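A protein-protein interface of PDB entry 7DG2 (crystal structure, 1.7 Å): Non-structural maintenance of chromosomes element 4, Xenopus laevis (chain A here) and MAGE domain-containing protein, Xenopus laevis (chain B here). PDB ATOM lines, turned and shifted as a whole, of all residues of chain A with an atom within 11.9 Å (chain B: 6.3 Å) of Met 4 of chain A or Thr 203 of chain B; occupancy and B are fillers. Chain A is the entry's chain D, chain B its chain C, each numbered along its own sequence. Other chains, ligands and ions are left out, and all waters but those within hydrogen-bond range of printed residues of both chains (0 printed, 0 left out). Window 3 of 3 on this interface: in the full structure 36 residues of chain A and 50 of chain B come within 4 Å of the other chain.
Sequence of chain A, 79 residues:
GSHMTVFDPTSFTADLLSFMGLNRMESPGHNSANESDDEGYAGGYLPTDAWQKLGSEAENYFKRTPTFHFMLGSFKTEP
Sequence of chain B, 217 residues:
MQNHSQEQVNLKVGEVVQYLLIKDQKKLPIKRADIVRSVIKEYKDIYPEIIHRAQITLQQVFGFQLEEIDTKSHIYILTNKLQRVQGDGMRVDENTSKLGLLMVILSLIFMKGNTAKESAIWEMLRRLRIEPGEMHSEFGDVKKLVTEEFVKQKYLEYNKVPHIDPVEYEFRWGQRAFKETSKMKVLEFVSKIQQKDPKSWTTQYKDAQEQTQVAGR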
ATOM      1  N   HIS A   3     -34.824 -14.668  31.827  1.00  0.00           N
ATOM      2  CA  HIS A   3     -34.247 -15.790  32.561  1.00  0.00           C
ATOM      3  C   HIS A   3     -33.241 -16.526  31.682  1.00  0.00           C
ATOM      4  O   HIS A   3     -33.593 -17.046  30.625  1.00  0.00           O
ATOM      5  CB  HIS A   3     -35.347 -16.744  33.038  1.00  0.00           C
ATOM      6  CG  HIS A   3     -34.863 -17.817  33.965  1.00  0.00           C
ATOM      7  ND1 HIS A   3     -34.020 -18.829  33.559  1.00  0.00           N
ATOM      8  CD2 HIS A   3     -35.123 -18.049  35.275  1.00  0.00           C
ATOM      9  CE1 HIS A   3     -33.770 -19.630  34.580  1.00  0.00           C
ATOM     10  NE2 HIS A   3     -34.431 -19.181  35.633  1.00  0.00           N
ATOM     11  N   MET A   4     -31.986 -16.560  32.121  1.00  0.00           N
ATOM     12  CA  MET A   4     -30.917 -17.248  31.414  1.00  0.00           C
ATOM     13  C   MET A   4     -30.414 -18.404  32.264  1.00  0.00           C
ATOM     14  O   MET A   4     -30.274 -18.276  33.485  1.00  0.00           O
ATOM     15  CB  MET A   4     -29.757 -16.298  31.093  1.00  0.00           C
ATOM     16  CG  MET A   4     -30.106 -15.180  30.125  1.00  0.00           C
ATOM     17  SD  MET A   4     -28.768 -13.986  29.936  1.00  0.00           S
ATOM     18  CE  MET A   4     -27.402 -15.063  29.498  1.00  0.00           C
ATOM     19  N   THR A   5     -30.151 -19.536  31.617  1.00  0.00           N
ATOM     20  CA  THR A   5     -29.563 -20.688  32.295  1.00  0.00           C
ATOM     21  C   THR A   5     -28.087 -20.388  32.539  1.00  0.00           C
ATOM     22  O   THR A   5     -27.261 -20.496  31.631  1.00  0.00           O
ATOM     23  CB  THR A   5     -29.749 -21.953  31.464  1.00  0.00           C
ATOM     24  OG1 THR A   5     -29.144 -21.765  30.177  1.00  0.00           O
ATOM     25  CG2 THR A   5     -31.238 -22.259  31.279  1.00  0.00           C
ATOM     26  N   VAL A   6     -27.756 -19.996  33.773  1.00  0.00           N
ATOM     27  CA  VAL A   6     -26.393 -19.630  34.145  1.00  0.00           C
ATOM     28  C   VAL A   6     -25.557 -20.887  34.341  1.00  0.00           C
ATOM     29  O   VAL A   6     -26.014 -21.869  34.940  1.00  0.00           O
ATOM     30  CB  VAL A   6     -26.404 -18.766  35.419  1.00  0.00           C
ATOM     31  CG1 VAL A   6     -24.985 -18.402  35.841  1.00  0.00           C
ATOM     32  CG2 VAL A   6     -27.238 -17.515  35.201  1.00  0.00           C
ATOM     33  N   PHE A   7     -24.317 -20.853  33.850  1.00  0.00           N
ATOM     34  CA  PHE A   7     -23.389 -21.976  33.967  1.00  0.00           C
ATOM     35  C   PHE A   7     -22.592 -21.859  35.259  1.00  0.00           C
ATOM     36  O   PHE A   7     -22.065 -20.788  35.571  1.00  0.00           O
ATOM     37  CB  PHE A   7     -22.439 -22.010  32.765  1.00  0.00           C
ATOM     38  CG  PHE A   7     -21.433 -23.135  32.799  1.00  0.00           C
ATOM     39  CD1 PHE A   7     -21.847 -24.457  32.715  1.00  0.00           C
ATOM     40  CD2 PHE A   7     -20.072 -22.867  32.873  1.00  0.00           C
ATOM     41  CE1 PHE A   7     -20.923 -25.493  32.725  1.00  0.00           C
ATOM     42  CE2 PHE A   7     -19.146 -23.895  32.876  1.00  0.00           C
ATOM     43  CZ  PHE A   7     -19.571 -25.211  32.801  1.00  0.00           C
ATOM     44  N   ASP A   8     -22.487 -22.971  35.994  1.00  0.00           N
ATOM     45  CA  ASP A   8     -21.760 -23.023  37.256  1.00  0.00           C
ATOM     46  C   ASP A   8     -20.399 -23.681  37.041  1.00  0.00           C
ATOM     47  O   ASP A   8     -20.322 -24.915  36.940  1.00  0.00           O
ATOM     48  CB  ASP A   8     -22.576 -23.797  38.298  1.00  0.00           C
ATOM     49  CG  ASP A   8     -21.898 -23.878  39.656  1.00  0.00           C
ATOM     50  OD1 ASP A   8     -20.783 -23.334  39.833  1.00  0.00           O
ATOM     51  OD2 ASP A   8     -22.494 -24.500  40.559  1.00  0.00           O
ATOM     52  N   SER B 200     -31.160 -28.931  28.766  1.00  0.00           N
ATOM     53  CA  SER B 200     -31.169 -28.336  30.103  1.00  0.00           C
ATOM     54  C   SER B 200     -30.636 -26.910  30.078  1.00  0.00           C
ATOM     55  O   SER B 200     -31.092 -26.054  30.845  1.00  0.00           O
ATOM     56  CB  SER B 200     -30.326 -29.170  31.077  1.00  0.00           C
ATOM     57  OG  SER B 200     -30.685 -30.537  31.049  1.00  0.00           O
ATOM     58  N   TRP B 201     -29.666 -26.641  29.210  1.00  0.00           N
ATOM     59  CA  TRP B 201     -29.019 -25.337  29.131  1.00  0.00           C
ATOM     60  C   TRP B 201     -29.663 -24.509  28.020  1.00  0.00           C
ATOM     61  O   TRP B 201     -29.070 -24.260  26.971  1.00  0.00           O
ATOM     62  CB  TRP B 201     -27.523 -25.513  28.886  1.00  0.00           C
ATOM     63  CG  TRP B 201     -26.812 -26.352  29.886  1.00  0.00           C
ATOM     64  CD1 TRP B 201     -26.456 -27.665  29.763  1.00  0.00           C
ATOM     65  CD2 TRP B 201     -26.339 -25.925  31.161  1.00  0.00           C
ATOM     66  NE1 TRP B 201     -25.787 -28.080  30.889  1.00  0.00           N
ATOM     67  CE2 TRP B 201     -25.703 -27.028  31.762  1.00  0.00           C
ATOM     68  CE3 TRP B 201     -26.387 -24.708  31.852  1.00  0.00           C
ATOM     69  CZ2 TRP B 201     -25.131 -26.957  33.027  1.00  0.00           C
ATOM     70  CZ3 TRP B 201     -25.824 -24.640  33.106  1.00  0.00           C
ATOM     71  CH2 TRP B 201     -25.201 -25.757  33.681  1.00  0.00           C
ATOM     72  N   THR B 202     -30.895 -24.059  28.293  1.00  0.00           N
ATOM     73  CA  THR B 202     -31.724 -23.411  27.276  1.00  0.00           C
ATOM     74  C   THR B 202     -30.987 -22.291  26.552  1.00  0.00           C
ATOM     75  O   THR B 202     -31.046 -22.186  25.321  1.00  0.00           O
ATOM     76  CB  THR B 202     -33.000 -22.859  27.919  1.00  0.00           C
ATOM     77  OG1 THR B 202     -33.719 -23.927  28.548  1.00  0.00           O
ATOM     78  CG2 THR B 202     -33.883 -22.218  26.873  1.00  0.00           C
ATOM     79  N   THR B 203     -30.297 -21.435  27.303  1.00  0.00           N
ATOM     80  CA  THR B 203     -29.619 -20.290  26.699  1.00  0.00           C
ATOM     81  C   THR B 203     -28.488 -20.734  25.779  1.00  0.00           C
ATOM     82  O   THR B 203     -28.368 -20.261  24.640  1.00  0.00           O
ATOM     83  CB  THR B 203     -29.082 -19.373  27.796  1.00  0.00           C
ATOM     84  OG1 THR B 203     -30.162 -18.969  28.655  1.00  0.00           O
ATOM     85  CG2 THR B 203     -28.426 -18.143  27.184  1.00  0.00           C
ATOM     86  N   GLN B 204     -27.636 -21.633  26.268  1.00  0.00           N
ATOM     87  CA  GLN B 204     -26.513 -22.104  25.467  1.00  0.00           C
ATOM     88  C   GLN B 204     -26.984 -22.984  24.315  1.00  0.00           C
ATOM     89  O   GLN B 204     -26.407 -22.943  23.220  1.00  0.00           O
ATOM     90  CB  GLN B 204     -25.528 -22.834  26.383  1.00  0.00           C
ATOM     91  CG  GLN B 204     -24.883 -21.910  27.451  1.00  0.00           C
ATOM     92  CD  GLN B 204     -25.730 -21.699  28.715  1.00  0.00           C
ATOM     93  OE1 GLN B 204     -26.884 -22.124  28.800  1.00  0.00           O
ATOM     94  NE2 GLN B 204     -25.138 -21.046  29.710  1.00  0.00           N
ATOM     95  N   TYR B 205     -28.048 -23.757  24.532  1.00  0.00           N
ATOM     96  CA  TYR B 205     -28.614 -24.559  23.453  1.00  0.00           C
ATOM     97  C   TYR B 205     -29.071 -23.686  22.291  1.00  0.00           C
ATOM     98  O   TYR B 205     -28.824 -24.013  21.127  1.00  0.00           O
ATOM     99  CB  TYR B 205     -29.779 -25.390  23.987  1.00  0.00           C
ATOM    100  CG  TYR B 205     -30.288 -26.416  23.016  1.00  0.00           C
ATOM    101  CD1 TYR B 205     -29.743 -27.691  22.982  1.00  0.00           C
ATOM    102  CD2 TYR B 205     -31.334 -26.126  22.152  1.00  0.00           C
ATOM    103  CE1 TYR B 205     -30.213 -28.641  22.102  1.00  0.00           C
ATOM    104  CE2 TYR B 205     -31.807 -27.069  21.269  1.00  0.00           C
ATOM    105  CZ  TYR B 205     -31.243 -28.324  21.248  1.00  0.00           C
ATOM    106  OH  TYR B 205     -31.717 -29.272  20.371  1.00  0.00           O
ATOM    107  N   LYS B 206     -29.750 -22.574  22.583  1.00  0.00           N
ATOM    108  CA  LYS B 206     -30.183 -21.706  21.494  1.00  0.00           C
ATOM    109  C   LYS B 206     -28.986 -21.087  20.783  1.00  0.00           C
ATOM    110  O   LYS B 206     -28.978 -20.980  19.553  1.00  0.00           O
ATOM    111  CB  LYS B 206     -31.130 -20.622  22.015  1.00  0.00           C
ATOM    112  CG  LYS B 206     -31.743 -19.776  20.904  1.00  0.00           C
ATOM    113  CD  LYS B 206     -32.972 -19.005  21.371  1.00  0.00           C
ATOM    114  CE  LYS B 206     -33.619 -18.251  20.208  1.00  0.00           C
ATOM    115  NZ  LYS B 206     -34.940 -17.661  20.581  1.00  0.00           N
ATOM    116  N   ASP B 207     -27.957 -20.693  21.542  1.00  0.00           N
ATOM    117  CA  ASP B 207     -26.759 -20.137  20.923  1.00  0.00           C
ATOM    118  C   ASP B 207     -26.076 -21.166  20.029  1.00  0.00           C
ATOM    119  O   ASP B 207     -25.557 -20.826  18.958  1.00  0.00           O
ATOM    120  CB  ASP B 207     -25.803 -19.631  22.001  1.00  0.00           C
ATOM    121  CG  ASP B 207     -24.607 -18.903  21.423  1.00  0.00           C
ATOM    122  OD1 ASP B 207     -24.786 -18.105  20.477  1.00  0.00           O
ATOM    123  OD2 ASP B 207     -23.489 -19.118  21.917  1.00  0.00           O
ATOM    124  N   ALA B 208     -26.091 -22.434  20.437  1.00  0.00           N
ATOM    125  CA  ALA B 208     -25.445 -23.477  19.647  1.00  0.00           C
ATOM    126  C   ALA B 208     -26.224 -23.813  18.382  1.00  0.00           C
ATOM    127  O   ALA B 208     -25.632 -24.315  17.420  1.00  0.00           O
ATOM    128  CB  ALA B 208     -25.252 -24.731  20.507  1.00  0.00           C
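N of Thr 202 of chain B lies within hydrogen-bond range of OG1 of Thr 5 of chain A (3.4 Å).
The side-chain amide oxygen of Gln 204 of chain B lies within hydrogen-bond range of the side-chain hydroxyl of Thr 5 of chain A (2.7 Å).
OG1 of Thr 203 of chain B sits at hydrogen-bond distance from N of Thr 5 of chain A (3.0 Å).
Thr 203 of chain B touches Met 4 of chain A.
Ser 200 of chain B touches Thr 5 of chain A (O to CG2, 3.8 Å).
Trp 201 of chain B touches Thr 5 of chain A.
Trp 201 of chain B touches Val 6 of chain A (CZ3 to O, 3.3 Å).
CA of Phe 7 of chain A touches CZ3 of Trp 201 of chain B, 3.7 Å away.
Of chain B, only Thr 203 comes within 4 Å of Met 4 of chain A.
Of the printed residues of chain B, Phe 7 of chain A touches Trp 201 (3.7 Å).
Asp 8 of chain A touches none of the printed residues of chain B.
Printed residues of chain A within 4 Å of Ser 200 of chain B: Thr 5.
Thr 203 of chain B touches two residues of chain A.
Gln 204 of chain B touches just one residue of chain A: Thr 5 (2.7 Å).
Lys 206 of chain B touches none of the printed residues of chain A.
The nearest residue of chain B that does not touch Met 4 of chain A is Gln 204 of chain B (6.2 Å).
The nearest residue of chain A that does not touch Thr 203 of chain B is His 3 of chain A (4.4 Å).
Of the 6 printed residues of chain A, 4 touch a printed residue of chain B.
Hydrophobic or aromatic side chains of chain A within 4 Å of the printed part of chain B: Met 4 and Phe 7.
Printed residues of chain B that touch a printed residue of chain A: Ser 200, Trp 201, Thr 202, Thr 203 and Gln 204.
Hydrophobic or aromatic side chains of chain B that line the printed part of chain A: Trp 201.
Among the printed residues, 8 pairs touch across the chains.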
